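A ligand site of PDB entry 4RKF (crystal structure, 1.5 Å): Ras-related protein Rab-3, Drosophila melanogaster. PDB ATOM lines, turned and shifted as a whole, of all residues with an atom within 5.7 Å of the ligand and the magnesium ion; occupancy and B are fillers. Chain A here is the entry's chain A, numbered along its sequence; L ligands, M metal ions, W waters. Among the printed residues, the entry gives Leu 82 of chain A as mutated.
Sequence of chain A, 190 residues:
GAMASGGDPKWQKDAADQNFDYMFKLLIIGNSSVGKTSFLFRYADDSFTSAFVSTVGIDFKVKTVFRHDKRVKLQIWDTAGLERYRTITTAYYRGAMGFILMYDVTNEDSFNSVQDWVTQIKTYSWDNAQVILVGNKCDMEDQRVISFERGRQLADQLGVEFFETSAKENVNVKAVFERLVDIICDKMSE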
ATOM      1  N   GLY A  30       9.363 -27.101  30.861  1.00  0.00           N
ATOM      2  CA  GLY A  30      10.733 -26.821  31.304  1.00  0.00           C
ATOM      3  C   GLY A  30      11.158 -25.432  30.900  1.00  0.00           C
ATOM      4  O   GLY A  30      10.461 -24.793  30.132  1.00  0.00           O
ATOM      5  N   ASN A  31      12.271 -24.975  31.455  1.00  0.00           N
ATOM      6  CA  ASN A  31      12.706 -23.599  31.225  1.00  0.00           C
ATOM      7  C   ASN A  31      12.923 -23.256  29.747  1.00  0.00           C
ATOM      8  O   ASN A  31      13.197 -24.141  28.913  1.00  0.00           O
ATOM      9  CB  ASN A  31      14.013 -23.301  32.000  1.00  0.00           C
ATOM     10  CG  ASN A  31      13.775 -23.063  33.480  1.00  0.00           C
ATOM     11  OD1 ASN A  31      12.732 -23.414  34.030  1.00  0.00           O
ATOM     12  ND2 ASN A  31      14.749 -22.439  34.134  1.00  0.00           N
ATOM     13  N   SER A  32      12.799 -21.971  29.423  1.00  0.00           N
ATOM     14  CA  SER A  32      13.151 -21.545  28.072  1.00  0.00           C
ATOM     15  C   SER A  32      14.621 -21.922  27.707  1.00  0.00           C
ATOM     16  O   SER A  32      15.523 -21.752  28.532  1.00  0.00           O
ATOM     17  CB  SER A  32      12.950 -20.021  27.937  1.00  0.00           C
ATOM     18  OG  SER A  32      13.321 -19.568  26.639  1.00  0.00           O
ATOM     19  N   SER A  33      14.768 -22.440  26.465  1.00  0.00           N
ATOM     20  CA  SER A  33      16.034 -22.805  25.783  1.00  0.00           C
ATOM     21  C   SER A  33      16.546 -24.209  26.084  1.00  0.00           C
ATOM     22  O   SER A  33      17.602 -24.584  25.570  1.00  0.00           O
ATOM     23  CB  SER A  33      17.178 -21.795  26.069  1.00  0.00           C
ATOM     24  OG  SER A  33      17.820 -22.056  27.326  1.00  0.00           O
ATOM     25  N   VAL A  34      15.813 -24.997  26.881  1.00  0.00           N
ATOM     26  CA  VAL A  34      16.333 -26.323  27.226  1.00  0.00           C
ATOM     27  C   VAL A  34      16.238 -27.336  26.095  1.00  0.00           C
ATOM     28  O   VAL A  34      16.925 -28.349  26.127  1.00  0.00           O
ATOM     29  CB  VAL A  34      15.658 -26.916  28.491  1.00  0.00           C
ATOM     30  CG1 VAL A  34      15.845 -25.969  29.690  1.00  0.00           C
ATOM     31  CG2 VAL A  34      14.201 -27.207  28.258  1.00  0.00           C
ATOM     32  N   GLY A  35      15.409 -27.031  25.096  1.00  0.00           N
ATOM     33  CA  GLY A  35      15.332 -27.825  23.878  1.00  0.00           C
ATOM     34  C   GLY A  35      13.995 -28.534  23.681  1.00  0.00           C
ATOM     35  O   GLY A  35      13.941 -29.582  23.027  1.00  0.00           O
ATOM     36  N   LYS A  36      12.904 -28.000  24.223  1.00  0.00           N
ATOM     37  CA  LYS A  36      11.593 -28.660  24.145  1.00  0.00           C
ATOM     38  C   LYS A  36      11.084 -28.752  22.704  1.00  0.00           C
ATOM     39  O   LYS A  36      10.683 -29.839  22.240  1.00  0.00           O
ATOM     40  CB  LYS A  36      10.573 -27.922  25.030  1.00  0.00           C
ATOM     41  CG  LYS A  36      10.970 -27.937  26.517  1.00  0.00           C
ATOM     42  CD  LYS A  36       9.950 -27.199  27.401  1.00  0.00           C
ATOM     43  CE  LYS A  36       9.745 -25.714  27.029  1.00  0.00           C
ATOM     44  NZ  LYS A  36      11.018 -24.899  27.106  1.00  0.00           N
ATOM     45  N   THR A  37      11.115 -27.631  21.999  1.00  0.00           N
ATOM     46  CA  THR A  37      10.695 -27.621  20.600  1.00  0.00           C
ATOM     47  C   THR A  37      11.584 -28.544  19.777  1.00  0.00           C
ATOM     48  O   THR A  37      11.112 -29.304  18.921  1.00  0.00           O
ATOM     49  CB  THR A  37      10.726 -26.177  20.066  1.00  0.00           C
ATOM     50  OG1 THR A  37       9.801 -25.428  20.870  1.00  0.00           O
ATOM     51  CG2 THR A  37      10.301 -26.076  18.603  1.00  0.00           C
ATOM     52  N   SER A  38      12.898 -28.492  20.044  1.00  0.00           N
ATOM     53  CA  SER A  38      13.811 -29.368  19.327  1.00  0.00           C
ATOM     54  C   SER A  38      13.527 -30.840  19.589  1.00  0.00           C
ATOM     55  O   SER A  38      13.666 -31.684  18.708  1.00  0.00           O
ATOM     56  CB  SER A  38      15.270 -29.076  19.696  1.00  0.00           C
ATOM     57  OG  SER A  38      15.652 -27.743  19.362  1.00  0.00           O
ATOM     58  N   PHE A  39      13.134 -31.151  20.824  1.00  0.00           N
ATOM     59  CA  PHE A  39      12.792 -32.531  21.191  1.00  0.00           C
ATOM     60  C   PHE A  39      11.637 -33.015  20.335  1.00  0.00           C
ATOM     61  O   PHE A  39      11.684 -34.116  19.767  1.00  0.00           O
ATOM     62  CB  PHE A  39      12.441 -32.570  22.674  1.00  0.00           C
ATOM     63  CG  PHE A  39      12.631 -33.927  23.328  1.00  0.00           C
ATOM     64  CD1 PHE A  39      13.895 -34.341  23.710  1.00  0.00           C
ATOM     65  CD2 PHE A  39      11.549 -34.750  23.583  1.00  0.00           C
ATOM     66  CE1 PHE A  39      14.109 -35.548  24.353  1.00  0.00           C
ATOM     67  CE2 PHE A  39      11.752 -35.990  24.211  1.00  0.00           C
ATOM     68  CZ  PHE A  39      13.025 -36.394  24.597  1.00  0.00           C
ATOM     69  N   PHE A  48      16.348 -31.185  12.952  1.00  0.00           N
ATOM     70  CA  PHE A  48      16.998 -30.342  13.947  1.00  0.00           C
ATOM     71  C   PHE A  48      17.355 -29.016  13.321  1.00  0.00           C
ATOM     72  O   PHE A  48      17.798 -28.970  12.161  1.00  0.00           O
ATOM     73  CB  PHE A  48      18.282 -31.016  14.483  1.00  0.00           C
ATOM     74  CG  PHE A  48      19.018 -30.167  15.485  1.00  0.00           C
ATOM     75  CD1 PHE A  48      18.601 -30.114  16.821  1.00  0.00           C
ATOM     76  CD2 PHE A  48      20.129 -29.426  15.112  1.00  0.00           C
ATOM     77  CE1 PHE A  48      19.284 -29.337  17.738  1.00  0.00           C
ATOM     78  CE2 PHE A  48      20.807 -28.635  16.049  1.00  0.00           C
ATOM     79  CZ  PHE A  48      20.380 -28.597  17.352  1.00  0.00           C
ATOM     80  N   THR A  49      17.199 -27.944  14.095  1.00  0.00           N
ATOM     81  CA  THR A  49      17.796 -26.671  13.733  1.00  0.00           C
ATOM     82  C   THR A  49      18.599 -26.105  14.897  1.00  0.00           C
ATOM     83  O   THR A  49      18.209 -26.223  16.065  1.00  0.00           O
ATOM     84  CB  THR A  49      16.750 -25.642  13.288  1.00  0.00           C
ATOM     85  OG1 THR A  49      17.429 -24.432  12.944  1.00  0.00           O
ATOM     86  CG2 THR A  49      15.745 -25.366  14.395  1.00  0.00           C
ATOM     87  N   SER A  50      19.719 -25.478  14.571  1.00  0.00           N
ATOM     88  CA  SER A  50      20.542 -24.799  15.565  1.00  0.00           C
ATOM     89  C   SER A  50      19.935 -23.461  15.992  1.00  0.00           C
ATOM     90  O   SER A  50      20.345 -22.896  16.999  1.00  0.00           O
ATOM     91  CB  SER A  50      21.937 -24.573  15.002  1.00  0.00           C
ATOM     92  OG  SER A  50      21.863 -23.800  13.807  1.00  0.00           O
ATOM     93  N   ALA A  51      18.980 -22.950  15.213  1.00  0.00           N
ATOM     94  CA  ALA A  51      18.371 -21.649  15.539  1.00  0.00           C
ATOM     95  C   ALA A  51      17.570 -21.762  16.830  1.00  0.00           C
ATOM     96  O   ALA A  51      16.943 -22.800  17.128  1.00  0.00           O
ATOM     97  CB  ALA A  51      17.476 -21.170  14.402  1.00  0.00           C
ATOM     98  N   PHE A  52      17.592 -20.688  17.627  1.00  0.00           N
ATOM     99  CA  PHE A  52      16.784 -20.622  18.832  1.00  0.00           C
ATOM    100  C   PHE A  52      15.696 -19.585  18.604  1.00  0.00           C
ATOM    101  O   PHE A  52      15.931 -18.389  18.683  1.00  0.00           O
ATOM    102  CB  PHE A  52      17.653 -20.275  20.047  1.00  0.00           C
ATOM    103  CG  PHE A  52      16.893 -20.098  21.325  1.00  0.00           C
ATOM    104  CD1 PHE A  52      15.654 -20.689  21.511  1.00  0.00           C
ATOM    105  CD2 PHE A  52      17.413 -19.305  22.337  1.00  0.00           C
ATOM    106  CE1 PHE A  52      14.940 -20.489  22.702  1.00  0.00           C
ATOM    107  CE2 PHE A  52      16.727 -19.117  23.529  1.00  0.00           C
ATOM    108  CZ  PHE A  52      15.479 -19.718  23.710  1.00  0.00           C
ATOM    109  N   VAL A  53      14.505 -20.066  18.309  1.00  0.00           N
ATOM    110  CA  VAL A  53      13.340 -19.199  18.186  1.00  0.00           C
ATOM    111  C   VAL A  53      12.375 -19.619  19.279  1.00  0.00           C
ATOM    112  O   VAL A  53      11.793 -20.710  19.209  1.00  0.00           O
ATOM    113  CB  VAL A  53      12.670 -19.304  16.795  1.00  0.00           C
ATOM    114  CG1 VAL A  53      11.429 -18.427  16.711  1.00  0.00           C
ATOM    115  CG2 VAL A  53      13.664 -18.932  15.671  1.00  0.00           C
ATOM    116  N   SER A  54      12.209 -18.781  20.299  1.00  0.00           N
ATOM    117  CA  SER A  54      11.321 -19.159  21.423  1.00  0.00           C
ATOM    118  C   SER A  54       9.897 -19.388  20.962  1.00  0.00           C
ATOM    119  O   SER A  54       9.384 -18.685  20.099  1.00  0.00           O
ATOM    120  CB  SER A  54      11.333 -18.096  22.524  1.00  0.00           C
ATOM    121  OG  SER A  54      12.432 -18.279  23.383  1.00  0.00           O
ATOM    122  N   THR A  55       9.279 -20.386  21.569  1.00  0.00           N
ATOM    123  CA  THR A  55       7.874 -20.693  21.385  1.00  0.00           C
ATOM    124  C   THR A  55       6.983 -19.654  22.047  1.00  0.00           C
ATOM    125  O   THR A  55       7.255 -19.224  23.164  1.00  0.00           O
ATOM    126  CB  THR A  55       7.599 -22.098  21.938  1.00  0.00           C
ATOM    127  OG1 THR A  55       8.506 -22.997  21.260  1.00  0.00           O
ATOM    128  CG2 THR A  55       6.180 -22.535  21.690  1.00  0.00           C
ATOM    129  N   ASP A  78       3.809 -28.708  22.878  1.00  0.00           N
ATOM    130  CA  ASP A  78       5.092 -28.074  23.098  1.00  0.00           C
ATOM    131  C   ASP A  78       4.862 -26.734  23.749  1.00  0.00           C
ATOM    132  O   ASP A  78       4.349 -25.821  23.110  1.00  0.00           O
ATOM    133  CB  ASP A  78       5.785 -27.933  21.746  1.00  0.00           C
ATOM    134  CG  ASP A  78       7.097 -27.170  21.829  1.00  0.00           C
ATOM    135  OD1 ASP A  78       7.696 -27.100  22.922  1.00  0.00           O
ATOM    136  OD2 ASP A  78       7.514 -26.664  20.748  1.00  0.00           O
ATOM    137  N   THR A  79       5.176 -26.635  25.031  1.00  0.00           N
ATOM    138  CA  THR A  79       4.888 -25.398  25.774  1.00  0.00           C
ATOM    139  C   THR A  79       6.029 -24.407  25.697  1.00  0.00           C
ATOM    140  O   THR A  79       7.199 -24.756  25.629  1.00  0.00           O
ATOM    141  CB  THR A  79       4.598 -25.672  27.268  1.00  0.00           C
ATOM    142  OG1 THR A  79       5.796 -26.160  27.917  1.00  0.00           O
ATOM    143  CG2 THR A  79       3.417 -26.633  27.451  1.00  0.00           C
ATOM    144  N   ALA A  80       5.683 -23.134  25.706  1.00  0.00           N
ATOM    145  CA  ALA A  80       6.687 -22.109  25.906  1.00  0.00           C
ATOM    146  C   ALA A  80       7.264 -22.212  27.301  1.00  0.00           C
ATOM    147  O   ALA A  80       6.513 -22.329  28.273  1.00  0.00           O
ATOM    148  CB  ALA A  80       6.081 -20.723  25.701  1.00  0.00           C
ATOM    149  N   GLY A  81       8.586 -22.104  27.416  1.00  0.00           N
ATOM    150  CA  GLY A  81       9.234 -22.024  28.712  1.00  0.00           C
ATOM    151  C   GLY A  81       9.317 -20.625  29.287  1.00  0.00           C
ATOM    152  O   GLY A  81       9.503 -20.479  30.499  1.00  0.00           O
ATOM    153  N   LEU A  82       9.219 -19.599  28.448  1.00  0.00           N
ATOM    154  CA  LEU A  82       9.329 -18.219  28.917  1.00  0.00           C
ATOM    155  C   LEU A  82       8.229 -17.902  29.931  1.00  0.00           C
ATOM    156  O   LEU A  82       7.059 -18.287  29.728  1.00  0.00           O
ATOM    157  CB  LEU A  82       9.257 -17.239  27.746  1.00  0.00           C
ATOM    158  CG  LEU A  82      10.505 -17.199  26.865  1.00  0.00           C
ATOM    159  CD1 LEU A  82      10.206 -16.357  25.633  1.00  0.00           C
ATOM    160  CD2 LEU A  82      11.658 -16.610  27.683  1.00  0.00           C
ATOM    161  N   ASN A 136      18.468 -32.802  28.790  1.00  0.00           N
ATOM    162  CA  ASN A 136      18.756 -32.690  27.358  1.00  0.00           C
ATOM    163  C   ASN A 136      20.117 -32.027  27.101  1.00  0.00           C
ATOM    164  O   ASN A 136      20.737 -31.439  28.017  1.00  0.00           O
ATOM    165  CB  ASN A 136      17.626 -31.920  26.666  1.00  0.00           C
ATOM    166  CG  ASN A 136      17.693 -31.949  25.151  1.00  0.00           C
ATOM    167  OD1 ASN A 136      17.925 -32.999  24.532  1.00  0.00           O
ATOM    168  ND2 ASN A 136      17.468 -30.809  24.526  1.00  0.00           N
ATOM    169  N   LYS A 137      20.557 -32.138  25.851  1.00  0.00           N
ATOM    170  CA  LYS A 137      21.801 -31.592  25.327  1.00  0.00           C
ATOM    171  C   LYS A 137      23.004 -32.376  25.844  1.00  0.00           C
ATOM    172  O   LYS A 137      24.079 -31.826  26.021  1.00  0.00           O
ATOM    173  CB  LYS A 137      21.966 -30.091  25.629  1.00  0.00           C
ATOM    174  CG  LYS A 137      20.742 -29.230  25.266  1.00  0.00           C
ATOM    175  CD  LYS A 137      21.121 -27.775  25.064  1.00  0.00           C
ATOM    176  CE  LYS A 137      19.886 -26.916  24.868  1.00  0.00           C
ATOM    177  NZ  LYS A 137      20.268 -25.457  24.937  1.00  0.00           N
ATOM    178  N   CYS A 138      22.829 -33.670  26.056  1.00  0.00           N
ATOM    179  CA  CYS A 138      23.931 -34.488  26.572  1.00  0.00           C
ATOM    180  C   CYS A 138      25.110 -34.623  25.587  1.00  0.00           C
ATOM    181  O   CYS A 138      26.169 -35.118  25.953  1.00  0.00           O
ATOM    182  CB  CYS A 138      23.422 -35.877  27.010  1.00  0.00           C
ATOM    183  SG  CYS A 138      22.876 -36.970  25.703  1.00  0.00           S
ATOM    184  N   ASP A 139      24.916 -34.175  24.345  1.00  0.00           N
ATOM    185  CA  ASP A 139      26.019 -34.108  23.384  1.00  0.00           C
ATOM    186  C   ASP A 139      27.043 -33.024  23.709  1.00  0.00           C
ATOM    187  O   ASP A 139      28.187 -33.093  23.233  1.00  0.00           O
ATOM    188  CB  ASP A 139      25.478 -33.890  21.968  1.00  0.00           C
ATOM    189  CG  ASP A 139      24.663 -32.607  21.859  1.00  0.00           C
ATOM    190  OD1 ASP A 139      23.526 -32.572  22.376  1.00  0.00           O
ATOM    191  OD2 ASP A 139      25.170 -31.656  21.232  1.00  0.00           O
ATOM    192  N   MET A 140      26.618 -32.035  24.495  1.00  0.00           N
ATOM    193  CA  MET A 140      27.468 -30.881  24.801  1.00  0.00           C
ATOM    194  C   MET A 140      28.360 -31.167  26.001  1.00  0.00           C
ATOM    195  O   MET A 140      28.305 -30.450  27.011  1.00  0.00           O
ATOM    196  CB  MET A 140      26.602 -29.646  25.063  1.00  0.00           C
ATOM    197  CG  MET A 140      25.673 -29.228  23.909  1.00  0.00           C
ATOM    198  SD  MET A 140      24.841 -27.613  24.145  1.00  0.00           S
ATOM    199  CE  MET A 140      26.255 -26.528  24.003  1.00  0.00           C
ATOM    200  N   THR A 165      19.222 -37.061  27.137  1.00  0.00           N
ATOM    201  CA  THR A 165      18.900 -37.051  25.716  1.00  0.00           C
ATOM    202  C   THR A 165      19.732 -36.028  24.967  1.00  0.00           C
ATOM    203  O   THR A 165      20.325 -35.100  25.529  1.00  0.00           O
ATOM    204  CB  THR A 165      17.403 -36.721  25.473  1.00  0.00           C
ATOM    205  OG1 THR A 165      17.125 -35.389  25.935  1.00  0.00           O
ATOM    206  CG2 THR A 165      16.488 -37.710  26.208  1.00  0.00           C
ATOM    207  N   SER A 166      19.742 -36.214  23.654  1.00  0.00           N
ATOM    208  CA  SER A 166      20.200 -35.197  22.725  1.00  0.00           C
ATOM    209  C   SER A 166      19.206 -35.071  21.565  1.00  0.00           C
ATOM    210  O   SER A 166      19.131 -35.948  20.706  1.00  0.00           O
ATOM    211  CB  SER A 166      21.598 -35.528  22.179  1.00  0.00           C
ATOM    212  OG  SER A 166      21.995 -34.491  21.288  1.00  0.00           O
ATOM    213  N   ALA A 167      18.438 -33.974  21.512  1.00  0.00           N
ATOM    214  CA  ALA A 167      17.652 -33.712  20.330  1.00  0.00           C
ATOM    215  C   ALA A 167      18.564 -33.540  19.136  1.00  0.00           C
ATOM    216  O   ALA A 167      18.217 -33.924  18.024  1.00  0.00           O
ATOM    217  CB  ALA A 167      16.797 -32.470  20.518  1.00  0.00           C
ATOM    218  N   LYS A 168      19.745 -32.947  19.371  1.00  0.00           N
ATOM    219  CA  LYS A 168      20.643 -32.638  18.257  1.00  0.00           C
ATOM    220  C   LYS A 168      21.181 -33.911  17.580  1.00  0.00           C
ATOM    221  O   LYS A 168      21.161 -34.011  16.341  1.00  0.00           O
ATOM    222  CB  LYS A 168      21.802 -31.753  18.719  1.00  0.00           C
ATOM    223  CG  LYS A 168      22.762 -31.377  17.604  1.00  0.00           C
ATOM    224  CD  LYS A 168      23.657 -30.198  18.025  1.00  0.00           C
ATOM    225  CE  LYS A 168      24.554 -29.699  16.895  1.00  0.00           C
ATOM    226  NZ  LYS A 168      25.604 -30.708  16.475  1.00  0.00           N
ATOM    227  N   GLU A 169      21.649 -34.877  18.367  1.00  0.00           N
ATOM    228  CA  GLU A 169      22.234 -36.104  17.801  1.00  0.00           C
ATOM    229  C   GLU A 169      21.302 -37.333  17.872  1.00  0.00           C
ATOM    230  O   GLU A 169      21.741 -38.473  17.591  1.00  0.00           O
ATOM    231  CB  GLU A 169      23.589 -36.414  18.482  1.00  0.00           C
ATOM    232  CG  GLU A 169      24.622 -35.302  18.228  1.00  0.00           C
ATOM    233  CD  GLU A 169      26.020 -35.635  18.723  1.00  0.00           C
ATOM    234  OE1 GLU A 169      26.237 -36.768  19.204  1.00  0.00           O
ATOM    235  OE2 GLU A 169      26.922 -34.759  18.596  1.00  0.00           O
HETATM  236  P1  LIG L   1      11.399 -22.052  24.492  1.00  0.00           P
HETATM  237  O1  LIG L   1      11.870 -20.630  24.676  1.00  0.00           O
HETATM  238  O2  LIG L   1      10.465 -22.273  23.340  1.00  0.00           O
HETATM  239  O3  LIG L   1      10.839 -22.563  25.800  1.00  0.00           O
HETATM  240  N1  LIG L   1      12.787 -22.901  24.187  1.00  0.00           N
HETATM  241  P2  LIG L   1      12.907 -24.499  23.901  1.00  0.00           P
HETATM  242  O4  LIG L   1      13.073 -25.238  25.156  1.00  0.00           O
HETATM  243  O5  LIG L   1      11.831 -24.917  22.978  1.00  0.00           O
HETATM  244  O6  LIG L   1      14.278 -24.622  23.123  1.00  0.00           O
HETATM  245  P3  LIG L   1      14.623 -24.914  21.600  1.00  0.00           P
HETATM  246  O7  LIG L   1      14.158 -26.267  21.219  1.00  0.00           O
HETATM  247  O8  LIG L   1      14.162 -23.747  20.802  1.00  0.00           O
HETATM  248  O9  LIG L   1      16.181 -24.991  21.612  1.00  0.00           O
HETATM  249  C1  LIG L   1      16.969 -23.907  22.149  1.00  0.00           C
HETATM  250  C2  LIG L   1      18.375 -24.000  21.571  1.00  0.00           C
HETATM  251  O10 LIG L   1      19.006 -25.250  21.997  1.00  0.00           O
HETATM  252  C3  LIG L   1      18.443 -24.010  20.053  1.00  0.00           C
HETATM  253  O11 LIG L   1      19.585 -23.224  19.656  1.00  0.00           O
HETATM  254  C4  LIG L   1      18.645 -25.486  19.677  1.00  0.00           C
HETATM  255  O12 LIG L   1      19.348 -25.718  18.470  1.00  0.00           O
HETATM  256  C5  LIG L   1      19.479 -25.955  20.853  1.00  0.00           C
HETATM  257  N2  LIG L   1      19.330 -27.386  21.171  1.00  0.00           N
HETATM  258  C6  LIG L   1      18.141 -28.037  21.442  1.00  0.00           C
HETATM  259  N3  LIG L   1      18.329 -29.308  21.753  1.00  0.00           N
HETATM  260  C7  LIG L   1      19.719 -29.488  21.693  1.00  0.00           C
HETATM  261  C8  LIG L   1      20.523 -30.636  21.938  1.00  0.00           C
HETATM  262  O13 LIG L   1      20.167 -31.772  22.239  1.00  0.00           O
HETATM  263  N4  LIG L   1      21.898 -30.379  21.810  1.00  0.00           N
HETATM  264  C9  LIG L   1      22.398 -29.161  21.442  1.00  0.00           C
HETATM  265  N5  LIG L   1      23.733 -29.089  21.346  1.00  0.00           N
HETATM  266  N6  LIG L   1      21.674 -28.078  21.201  1.00  0.00           N
HETATM  267  C10 LIG L   1      20.333 -28.301  21.365  1.00  0.00           C
HETATM  268 MG    MG M   1      10.194 -23.874  22.144  1.00  0.00          MG
HETATM  269  O   HOH W   1      11.542 -23.078  20.711  1.00  0.00           O
HETATM  270  O   HOH W   2      21.380 -21.767  21.430  1.00  0.00           O
HETATM  271  O   HOH W   3       8.936 -24.875  23.538  1.00  0.00           O
HETATM  272  O   HOH W   4       9.101 -19.675  25.282  1.00  0.00           O
HETATM  273  O   HOH W   5      14.380 -23.037  18.218  1.00  0.00           O
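The side-chain amino group of Lys 137 lies within hydrogen-bond range of the backbone carbonyl oxygen of Ser 33 (2.9 Å). The backbone NH (N) of Ala 167 sits at hydrogen-bond distance from the side-chain amide oxygen (OD1) of Asn 136, 3.2 Å away. The side-chain hydroxyl (OG) of Ser 166 is in hydrogen-bond range of the side-chain carboxylate (OD1) of Asp 139 (2.7 Å). OG of Ser 166 sits at hydrogen-bond distance from N of Glu 169, at 3.0 Å. OG1 of Thr 49 lies within hydrogen-bond range of N of Ala 51 (3.1 Å). The backbone NH (N) of Lys 168 sits close to the side-chain hydroxyl (OG) of Ser 166, at 3.3 Å. The side-chain hydroxyl (OG1) of Thr 37 lies close to the side-chain carboxylate (OD2) of Asp 78 (2.6 Å). The backbone carbonyl oxygen (O) of Val 34 is in hydrogen-bond range of the side-chain amide nitrogen (ND2) of Asn 136 (3.0 Å).
O10 of the ligand is in hydrogen-bond range of NZ of Lys 137, at 3.2 Å. An oxygen (O11) of the ligand is in hydrogen-bond range of the backbone carbonyl oxygen (O) of Ser 50. An oxygen (O4) of the ligand sits at hydrogen-bond distance from the backbone NH (N) of Lys 36. An oxygen (O4) of the ligand sits at hydrogen-bond distance from the backbone NH (N) of Gly 35 (2.9 Å). An oxygen (O7) of the ligand lies within hydrogen-bond range of the backbone NH (N) of Ser 38 (2.8 Å). O2 of the ligand sits close to N of Thr 55 (2.8 Å). The side-chain sulfur of Met 140 sits close to a nitrogen (N5) of the ligand. An oxygen (O1) of the ligand lies within hydrogen-bond range of the side-chain hydroxyl (OG) of Ser 54. A nitrogen (N3) of the ligand is in hydrogen-bond range of the side-chain amide nitrogen (ND2) of Asn 136 (3.3 Å). An oxygen (O4) of the ligand lies within hydrogen-bond range of the backbone NH of Val 34. An oxygen (O7) of the ligand sits at hydrogen-bond distance from the backbone NH (N) of Thr 37. An oxygen (O12) of the ligand sits at hydrogen-bond distance from the backbone carbonyl oxygen (O) of Thr 49 (2.7 Å). OD1 of Asp 139 sits at hydrogen-bond distance from N4 of the ligand. OG of Ser 166 is in hydrogen-bond range of O13 of the ligand, at 3.4 Å. An oxygen (O13) of the ligand sits at hydrogen-bond distance from the backbone NH (N) of Ala 167 (2.9 Å). N of Lys 168 lies within hydrogen-bond range of O13 of the ligand (3.1 Å). An oxygen (O1) of the ligand lies within hydrogen-bond range of the side-chain hydroxyl (OG) of Ser 32, 2.7 Å away. The side-chain hydroxyl (OG) of Ser 38 sits at hydrogen-bond distance from an oxygen (O7) of the ligand (2.8 Å). The side-chain amino group (NZ) of Lys 36 is in salt-bridge range of an oxygen (O3) of the ligand (2.7 Å). An oxygen (O3) of the ligand sits at hydrogen-bond distance from the backbone NH of Gly 81.
The magnesium ion is bound by O2 of the ligand, 2.0 Å away. The magnesium ion is bound by the side-chain hydroxyl (OG1) of Thr 37. The magnesium ion is bound by OG1 of Thr 55 (2.1 Å). O5 of the ligand is bound to the magnesium ion, at 2.1 Å. The magnesium ion is bound by water W1 (2.1 Å). Water W3 is bound to the magnesium ion (2.1 Å).
Two residues have an atom within 4 Å of the magnesium ion: Thr 37 and Thr 55. The nearest printed residue that does not touch the magnesium ion is Asp 78 (4.1 Å).
N of Ser 33 lies close to N1 of the ligand (3.1 Å). Asn 31 touches the ligand. Phe 48 touches the ligand (CZ to O12, 3.3 Å). Ala 51 touches the ligand. Phe 52 touches the ligand (CD1 to O8, 3.5 Å). C of Ala 80 touches O3 of the ligand (3.9 Å). Hydrophobic or aromatic side chains within 4 Å of the ligand: Val 34, Phe 48, Phe 52, Met 140 and Ala 167. 24 residues have an atom within 4 Å of the ligand: Asn 31, Ser 32, Ser 33, Val 34, Gly 35, Lys 36, Thr 37, Ser 38, Phe 48, Thr 49, Ser 50, Ala 51, Phe 52, Ser 54, Thr 55, Ala 80, Gly 81, Asn 136, Lys 137, Asp 139, Met 140, Ser 166, Ala 167 and Lys 168. The nearest printed residue that does not touch the ligand is Val 53 (4.2 Å).
Water W3 bridges OD1 of Asp 78 (2.6 Å) and O of Thr 79 (2.7 Å). Water W1 lies within hydrogen-bond range of O8 of the ligand (2.7 Å) and O of Val 53 (2.8 Å). Water W5 lies within hydrogen-bond range of an oxygen (O8) of the ligand, the backbone carbonyl oxygen (O) of Ala 51 and the backbone NH (N) of Val 53. Water W4 lies within hydrogen-bond range of O of Thr 55 (2.8 Å), O1 of the ligand (3.0 Å), N of Leu 82 (3.2 Å) and N of Gly 81 (3.3 Å).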
